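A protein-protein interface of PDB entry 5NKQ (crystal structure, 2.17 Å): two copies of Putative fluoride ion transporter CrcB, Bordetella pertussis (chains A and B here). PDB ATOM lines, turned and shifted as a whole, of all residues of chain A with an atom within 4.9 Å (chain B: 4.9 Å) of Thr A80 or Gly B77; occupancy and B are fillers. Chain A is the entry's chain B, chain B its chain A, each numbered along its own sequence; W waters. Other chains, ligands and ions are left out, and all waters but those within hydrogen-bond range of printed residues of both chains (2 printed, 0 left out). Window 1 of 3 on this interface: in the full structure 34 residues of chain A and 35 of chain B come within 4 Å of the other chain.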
ATOM      1  N   ARG A  23     -20.130 -14.713   4.564  1.00  0.00           N
ATOM      2  CA  ARG A  23     -20.009 -15.181   3.186  1.00  0.00           C
ATOM      3  C   ARG A  23     -21.372 -15.532   2.600  1.00  0.00           C
ATOM      4  O   ARG A  23     -21.650 -15.228   1.434  1.00  0.00           O
ATOM      5  CB  ARG A  23     -19.069 -16.384   3.116  1.00  0.00           C
ATOM      6  CG  ARG A  23     -19.199 -17.193   1.833  1.00  0.00           C
ATOM      7  CD  ARG A  23     -18.097 -18.229   1.703  1.00  0.00           C
ATOM      8  NE  ARG A  23     -17.940 -19.022   2.918  1.00  0.00           N
ATOM      9  CZ  ARG A  23     -18.662 -20.099   3.205  1.00  0.00           C
ATOM     10  NH1 ARG A  23     -19.601 -20.512   2.362  1.00  0.00           N
ATOM     11  NH2 ARG A  23     -18.451 -20.760   4.334  1.00  0.00           N
ATOM     12  N   ALA A  42     -16.342 -12.119  -1.122  1.00  0.00           N
ATOM     13  CA  ALA A  42     -15.915 -12.802   0.093  1.00  0.00           C
ATOM     14  C   ALA A  42     -14.442 -13.183   0.027  1.00  0.00           C
ATOM     15  O   ALA A  42     -13.711 -13.041   1.014  1.00  0.00           O
ATOM     16  CB  ALA A  42     -16.783 -14.038   0.330  1.00  0.00           C
ATOM     17  N   ASN A  43     -13.984 -13.663  -1.132  1.00  0.00           N
ATOM     18  CA  ASN A  43     -12.586 -14.060  -1.265  1.00  0.00           C
ATOM     19  C   ASN A  43     -11.665 -12.847  -1.331  1.00  0.00           C
ATOM     20  O   ASN A  43     -10.557 -12.874  -0.785  1.00  0.00           O
ATOM     21  CB  ASN A  43     -12.404 -14.942  -2.500  1.00  0.00           C
ATOM     22  CG  ASN A  43     -13.003 -16.324  -2.324  1.00  0.00           C
ATOM     23  OD1 ASN A  43     -13.197 -16.789  -1.201  1.00  0.00           O
ATOM     24  ND2 ASN A  43     -13.291 -16.990  -3.436  1.00  0.00           N
ATOM     25  N   GLY A  46     -11.617 -11.327   2.215  1.00  0.00           N
ATOM     26  CA  GLY A  46     -10.854 -12.226   3.063  1.00  0.00           C
ATOM     27  C   GLY A  46      -9.379 -12.247   2.713  1.00  0.00           C
ATOM     28  O   GLY A  46      -8.523 -12.356   3.594  1.00  0.00           O
ATOM     29  N   GLY A  47      -9.062 -12.143   1.421  1.00  0.00           N
ATOM     30  CA  GLY A  47      -7.668 -12.055   1.020  1.00  0.00           C
ATOM     31  C   GLY A  47      -7.009 -10.777   1.502  1.00  0.00           C
ATOM     32  O   GLY A  47      -5.844 -10.782   1.907  1.00  0.00           O
ATOM     33  N   LEU A  76     -11.600 -15.700   8.888  1.00  0.00           N
ATOM     34  CA  LEU A  76     -11.171 -15.611   7.495  1.00  0.00           C
ATOM     35  C   LEU A  76     -11.210 -16.967   6.806  1.00  0.00           C
ATOM     36  O   LEU A  76     -11.491 -17.041   5.604  1.00  0.00           O
ATOM     37  CB  LEU A  76      -9.772 -15.007   7.417  1.00  0.00           C
ATOM     38  CG  LEU A  76      -9.683 -13.600   8.011  1.00  0.00           C
ATOM     39  CD1 LEU A  76      -8.263 -13.071   7.945  1.00  0.00           C
ATOM     40  CD2 LEU A  76     -10.651 -12.662   7.303  1.00  0.00           C
ATOM     41  N   GLY A  77     -10.938 -18.045   7.548  1.00  0.00           N
ATOM     42  CA  GLY A  77     -11.060 -19.376   6.978  1.00  0.00           C
ATOM     43  C   GLY A  77     -12.493 -19.747   6.650  1.00  0.00           C
ATOM     44  O   GLY A  77     -12.736 -20.599   5.796  1.00  0.00           O
ATOM     45  N   GLY A  78     -13.456 -19.121   7.323  1.00  0.00           N
ATOM     46  CA  GLY A  78     -14.860 -19.355   7.050  1.00  0.00           C
ATOM     47  C   GLY A  78     -15.411 -18.367   6.046  1.00  0.00           C
ATOM     48  O   GLY A  78     -16.348 -18.679   5.307  1.00  0.00           O
ATOM     49  N   LEU A  79     -14.820 -17.171   6.002  1.00  0.00           N
ATOM     50  CA  LEU A  79     -15.286 -16.147   5.072  1.00  0.00           C
ATOM     51  C   LEU A  79     -14.935 -16.506   3.633  1.00  0.00           C
ATOM     52  O   LEU A  79     -15.775 -16.392   2.732  1.00  0.00           O
ATOM     53  CB  LEU A  79     -14.695 -14.788   5.449  1.00  0.00           C
ATOM     54  CG  LEU A  79     -14.993 -13.632   4.492  1.00  0.00           C
ATOM     55  CD1 LEU A  79     -16.493 -13.397   4.377  1.00  0.00           C
ATOM     56  CD2 LEU A  79     -14.279 -12.367   4.946  1.00  0.00           C
ATOM     57  N   THR A  80     -13.699 -16.932   3.392  1.00  0.00           N
ATOM     58  CA  THR A  80     -13.297 -17.312   2.048  1.00  0.00           C
ATOM     59  C   THR A  80     -13.700 -18.756   1.765  1.00  0.00           C
ATOM     60  O   THR A  80     -14.119 -19.498   2.655  1.00  0.00           O
ATOM     61  CB  THR A  80     -11.792 -17.129   1.860  1.00  0.00           C
ATOM     62  OG1 THR A  80     -11.084 -17.963   2.784  1.00  0.00           O
ATOM     63  CG2 THR A  80     -11.405 -15.676   2.092  1.00  0.00           C
ATOM     64  N   THR A  81     -13.579 -19.150   0.500  1.00  0.00           N
ATOM     65  CA  THR A  81     -13.970 -20.491   0.093  1.00  0.00           C
ATOM     66  C   THR A  81     -13.274 -20.842  -1.213  1.00  0.00           C
ATOM     67  O   THR A  81     -13.202 -20.018  -2.129  1.00  0.00           O
ATOM     68  CB  THR A  81     -15.494 -20.610  -0.068  1.00  0.00           C
ATOM     69  OG1 THR A  81     -15.818 -21.873  -0.662  1.00  0.00           O
ATOM     70  CG2 THR A  81     -16.036 -19.483  -0.942  1.00  0.00           C
ATOM     71  N   PHE A  82     -12.754 -22.065  -1.283  1.00  0.00           N
ATOM     72  CA  PHE A  82     -12.188 -22.592  -2.516  1.00  0.00           C
ATOM     73  C   PHE A  82     -13.128 -23.552  -3.229  1.00  0.00           C
ATOM     74  O   PHE A  82     -13.143 -23.584  -4.464  1.00  0.00           O
ATOM     75  CB  PHE A  82     -10.861 -23.309  -2.229  1.00  0.00           C
ATOM     76  CG  PHE A  82      -9.819 -23.104  -3.292  1.00  0.00           C
ATOM     77  CD1 PHE A  82      -9.923 -23.740  -4.517  1.00  0.00           C
ATOM     78  CD2 PHE A  82      -8.731 -22.279  -3.061  1.00  0.00           C
ATOM     79  CE1 PHE A  82      -8.964 -23.552  -5.496  1.00  0.00           C
ATOM     80  CE2 PHE A  82      -7.769 -22.087  -4.033  1.00  0.00           C
ATOM     81  CZ  PHE A  82      -7.885 -22.725  -5.253  1.00  0.00           C
ATOM     82  N   SER A  83     -13.917 -24.322  -2.475  1.00  0.00           N
ATOM     83  CA  SER A  83     -14.831 -25.280  -3.086  1.00  0.00           C
ATOM     84  C   SER A  83     -15.947 -24.576  -3.849  1.00  0.00           C
ATOM     85  O   SER A  83     -16.293 -24.984  -4.964  1.00  0.00           O
ATOM     86  CB  SER A  83     -15.408 -26.205  -2.015  1.00  0.00           C
ATOM     87  OG  SER A  83     -15.875 -25.464  -0.899  1.00  0.00           O
ATOM     88  N   ALA B  71     -23.926 -28.703   4.470  1.00  0.00           N
ATOM     89  CA  ALA B  71     -22.867 -29.487   3.845  1.00  0.00           C
ATOM     90  C   ALA B  71     -21.957 -28.637   2.961  1.00  0.00           C
ATOM     91  O   ALA B  71     -20.731 -28.703   3.087  1.00  0.00           O
ATOM     92  CB  ALA B  71     -23.476 -30.629   3.026  1.00  0.00           C
ATOM     93  N   VAL B  72     -22.536 -27.844   2.061  1.00  0.00           N
ATOM     94  CA  VAL B  72     -21.747 -27.092   1.090  1.00  0.00           C
ATOM     95  C   VAL B  72     -21.403 -25.717   1.647  1.00  0.00           C
ATOM     96  O   VAL B  72     -20.226 -25.392   1.843  1.00  0.00           O
ATOM     97  CB  VAL B  72     -22.486 -26.966  -0.254  1.00  0.00           C
ATOM     98  CG1 VAL B  72     -21.616 -26.243  -1.267  1.00  0.00           C
ATOM     99  CG2 VAL B  72     -22.890 -28.339  -0.768  1.00  0.00           C
ATOM    100  N   THR B  73     -22.428 -24.895   1.894  1.00  0.00           N
ATOM    101  CA  THR B  73     -22.191 -23.551   2.409  1.00  0.00           C
ATOM    102  C   THR B  73     -21.500 -23.595   3.767  1.00  0.00           C
ATOM    103  O   THR B  73     -20.614 -22.778   4.049  1.00  0.00           O
ATOM    104  CB  THR B  73     -23.512 -22.784   2.504  1.00  0.00           C
ATOM    105  OG1 THR B  73     -24.173 -22.810   1.233  1.00  0.00           O
ATOM    106  CG2 THR B  73     -23.266 -21.338   2.911  1.00  0.00           C
ATOM    107  N   GLY B  74     -21.882 -24.546   4.613  1.00  0.00           N
ATOM    108  CA  GLY B  74     -21.284 -24.671   5.926  1.00  0.00           C
ATOM    109  C   GLY B  74     -20.008 -25.488   5.938  1.00  0.00           C
ATOM    110  O   GLY B  74     -18.911 -24.927   6.009  1.00  0.00           O
ATOM    111  N   PHE B  75     -20.142 -26.814   5.849  1.00  0.00           N
ATOM    112  CA  PHE B  75     -18.998 -27.701   6.043  1.00  0.00           C
ATOM    113  C   PHE B  75     -17.909 -27.449   5.006  1.00  0.00           C
ATOM    114  O   PHE B  75     -16.754 -27.175   5.352  1.00  0.00           O
ATOM    115  CB  PHE B  75     -19.453 -29.161   6.003  1.00  0.00           C
ATOM    116  CG  PHE B  75     -18.327 -30.147   6.125  1.00  0.00           C
ATOM    117  CD1 PHE B  75     -17.724 -30.379   7.349  1.00  0.00           C
ATOM    118  CD2 PHE B  75     -17.872 -30.839   5.016  1.00  0.00           C
ATOM    119  CE1 PHE B  75     -16.685 -31.285   7.467  1.00  0.00           C
ATOM    120  CE2 PHE B  75     -16.835 -31.747   5.126  1.00  0.00           C
ATOM    121  CZ  PHE B  75     -16.240 -31.970   6.353  1.00  0.00           C
ATOM    122  N   LEU B  76     -18.257 -27.543   3.722  1.00  0.00           N
ATOM    123  CA  LEU B  76     -17.254 -27.351   2.679  1.00  0.00           C
ATOM    124  C   LEU B  76     -16.766 -25.909   2.627  1.00  0.00           C
ATOM    125  O   LEU B  76     -15.623 -25.658   2.227  1.00  0.00           O
ATOM    126  CB  LEU B  76     -17.819 -27.783   1.328  1.00  0.00           C
ATOM    127  CG  LEU B  76     -18.148 -29.274   1.263  1.00  0.00           C
ATOM    128  CD1 LEU B  76     -18.758 -29.639  -0.079  1.00  0.00           C
ATOM    129  CD2 LEU B  76     -16.902 -30.103   1.540  1.00  0.00           C
ATOM    130  N   GLY B  77     -17.608 -24.954   3.027  1.00  0.00           N
ATOM    131  CA  GLY B  77     -17.172 -23.574   3.120  1.00  0.00           C
ATOM    132  C   GLY B  77     -16.234 -23.310   4.278  1.00  0.00           C
ATOM    133  O   GLY B  77     -15.500 -22.316   4.255  1.00  0.00           O
ATOM    134  N   GLY B  78     -16.245 -24.170   5.290  1.00  0.00           N
ATOM    135  CA  GLY B  78     -15.313 -24.046   6.392  1.00  0.00           C
ATOM    136  C   GLY B  78     -14.086 -24.909   6.193  1.00  0.00           C
ATOM    137  O   GLY B  78     -13.022 -24.632   6.754  1.00  0.00           O
ATOM    138  N   LEU B  79     -14.225 -25.960   5.381  1.00  0.00           N
ATOM    139  CA  LEU B  79     -13.102 -26.857   5.123  1.00  0.00           C
ATOM    140  C   LEU B  79     -12.096 -26.224   4.170  1.00  0.00           C
ATOM    141  O   LEU B  79     -10.888 -26.230   4.435  1.00  0.00           O
ATOM    142  CB  LEU B  79     -13.612 -28.184   4.564  1.00  0.00           C
ATOM    143  CG  LEU B  79     -12.536 -29.160   4.090  1.00  0.00           C
ATOM    144  CD1 LEU B  79     -11.598 -29.536   5.234  1.00  0.00           C
ATOM    145  CD2 LEU B  79     -13.177 -30.394   3.481  1.00  0.00           C
ATOM    146  N   THR B  80     -12.569 -25.684   3.052  1.00  0.00           N
ATOM    147  CA  THR B  80     -11.675 -25.045   2.099  1.00  0.00           C
ATOM    148  C   THR B  80     -11.363 -23.619   2.543  1.00  0.00           C
ATOM    149  O   THR B  80     -12.005 -23.060   3.433  1.00  0.00           O
ATOM    150  CB  THR B  80     -12.285 -25.044   0.699  1.00  0.00           C
ATOM    151  OG1 THR B  80     -13.483 -24.257   0.695  1.00  0.00           O
ATOM    152  CG2 THR B  80     -12.613 -26.464   0.272  1.00  0.00           C
ATOM    153  N   THR B  81     -10.353 -23.026   1.910  1.00  0.00           N
ATOM    154  CA  THR B  81      -9.950 -21.675   2.266  1.00  0.00           C
ATOM    155  C   THR B  81      -9.223 -21.039   1.091  1.00  0.00           C
ATOM    156  O   THR B  81      -8.374 -21.671   0.457  1.00  0.00           O
ATOM    157  CB  THR B  81      -9.054 -21.667   3.514  1.00  0.00           C
ATOM    158  OG1 THR B  81      -8.547 -20.344   3.732  1.00  0.00           O
ATOM    159  CG2 THR B  81      -7.893 -22.640   3.357  1.00  0.00           C
ATOM    160  N   PHE B  82      -9.577 -19.790   0.801  1.00  0.00           N
ATOM    161  CA  PHE B  82      -8.870 -18.989  -0.188  1.00  0.00           C
ATOM    162  C   PHE B  82      -7.896 -18.006   0.443  1.00  0.00           C
ATOM    163  O   PHE B  82      -6.836 -17.741  -0.135  1.00  0.00           O
ATOM    164  CB  PHE B  82      -9.868 -18.218  -1.059  1.00  0.00           C
ATOM    165  CG  PHE B  82      -9.489 -18.156  -2.510  1.00  0.00           C
ATOM    166  CD1 PHE B  82      -8.401 -17.407  -2.924  1.00  0.00           C
ATOM    167  CD2 PHE B  82     -10.229 -18.837  -3.462  1.00  0.00           C
ATOM    168  CE1 PHE B  82      -8.052 -17.346  -4.260  1.00  0.00           C
ATOM    169  CE2 PHE B  82      -9.887 -18.779  -4.799  1.00  0.00           C
ATOM    170  CZ  PHE B  82      -8.796 -18.033  -5.199  1.00  0.00           C
ATOM    171  N   SER B  83      -8.229 -17.474   1.621  1.00  0.00           N
ATOM    172  CA  SER B  83      -7.355 -16.514   2.287  1.00  0.00           C
ATOM    173  C   SER B  83      -6.060 -17.171   2.744  1.00  0.00           C
ATOM    174  O   SER B  83      -4.969 -16.632   2.523  1.00  0.00           O
ATOM    175  CB  SER B  83      -8.084 -15.880   3.472  1.00  0.00           C
ATOM    176  OG  SER B  83      -8.601 -16.873   4.342  1.00  0.00           O
HETATM  177  O   HOH W   1      -7.715 -18.069   6.623  1.00  0.00           O
HETATM  178  O   HOH W   2     -18.436 -24.502  -0.380  1.00  0.00           O
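Leu A76 touches Ser B83, and with the chains exchanged Ser A83 touches Leu B76.
Gly A77 touches Thr B80, and with the chains exchanged Thr A80 touches Gly B77.
Thr A80 touches Ser B83, and with the chains exchanged Ser A83 touches Thr B80.
Phe B82 touches its own counterpart, Phe A82.
Of the 19 pairs that touch across the chains among the printed residues, 14 have their exchanged pair printed and touching as well.
O of Val B72 is in hydrogen-bond range of N of Gly B77, at 2.9 Å.
The backbone carbonyl oxygen (O) of Leu A79 sits close to the guanidinium group (NE) of Arg A23 (3.4 Å).
OG1 of Thr A80 lies within hydrogen-bond range of O of Leu A76, at 3.0 Å.
The backbone NH of Thr A81 is in hydrogen-bond range of the side-chain amide oxygen of Asn A43, at 2.9 Å.
The backbone carbonyl oxygen (O) of Ala B71 lies within hydrogen-bond range of the backbone NH (N) of Leu B76 (2.8 Å).
O of Leu B76 sits at hydrogen-bond distance from OG1 of Thr B80 (3.0 Å).
Of the 13 printed residues of chain B, 7 touch a printed residue of chain A.
Hydrophobic or aromatic side chains of chain B within 4 Å of the printed part of chain A: Leu B76 and Phe B82.
Of the 13 printed residues of chain A, 10 touch a printed residue of chain B.
Printed residues of chain A that touch a printed residue of chain B: Arg A23, Asn A43, Gly A46, Leu A76, Gly A77, Gly A78, Thr A80, Thr A81, Phe A82 and Ser A83.
Hydrophobic or aromatic side chains of chain A that line the printed part of chain B: Leu A76 and Phe A82.
Among the printed residues, 19 pairs touch across the chains.
Printed residues of chain B within 4 Å of Gly A46: Ser B83.
Printed residues of chain B within 4 Å of Gly A78: Gly B77.
Printed residues of chain B within 4 Å of Thr A80: Gly B77, Thr B81, Phe B82 and Ser B83.
Printed residues of chain B within 4 Å of Thr A81: Thr B80 (3.6 Å) and Phe B82 (3.5 Å).
Printed residues of chain B within 4 Å of Phe A82: Thr B80, Thr B81 and Phe B82.
Of the printed residues of chain A, Gly B77 touches Arg A23, Gly A77, Gly A78 and Thr A80.
Water W1 lies within hydrogen-bond range of OG of Ser B83 and N of Gly A77.
Water W2 bridges OG of Ser A83 and O of Val B72.
Among the printed residues, merely in contact across the chains: Thr A81 with Phe B82, Thr A80 with Gly B77, Gly A46 with Ser B83, Asn A43 with Phe B82, Phe A82 with Thr B81, Gly A77 with Gly B77, Thr A81 with Thr B80, Thr A80 with Thr B81, Phe A82 with Phe B82 and Gly A78 with Gly B77.
The backbone carbonyl oxygen (O) of Thr B73 is in hydrogen-bond range of the guanidinium group (NH2) of Arg A23 (3.0 Å).
The backbone carbonyl oxygen (O) of Leu B76 lies within hydrogen-bond range of the side-chain hydroxyl (OG) of Ser A83.
The backbone carbonyl oxygen (O) of Leu A76 is in hydrogen-bond range of the side-chain hydroxyl (OG) of Ser B83, at 3.2 Å.
The backbone NH (N) of Ser B83 lies within hydrogen-bond range of the side-chain hydroxyl (OG1) of Thr A80, at 3.1 Å.
The side-chain hydroxyl (OG1) of Thr A80 is in hydrogen-bond range of the backbone NH (N) of Phe B82 (3.1 Å).
OG of Ser A83 is in hydrogen-bond range of OG1 of Thr B80 (3.1 Å).
N of Phe A82 is in hydrogen-bond range of OG1 of Thr B80 (3.0 Å).
The backbone carbonyl oxygen (O) of Gly A77 sits close to the backbone carbonyl oxygen (O) of Thr B80 (3.5 Å).
The backbone carbonyl oxygen (O) of Gly B77 sits close to the guanidinium group (NH2) of Arg A23 (3.3 Å).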
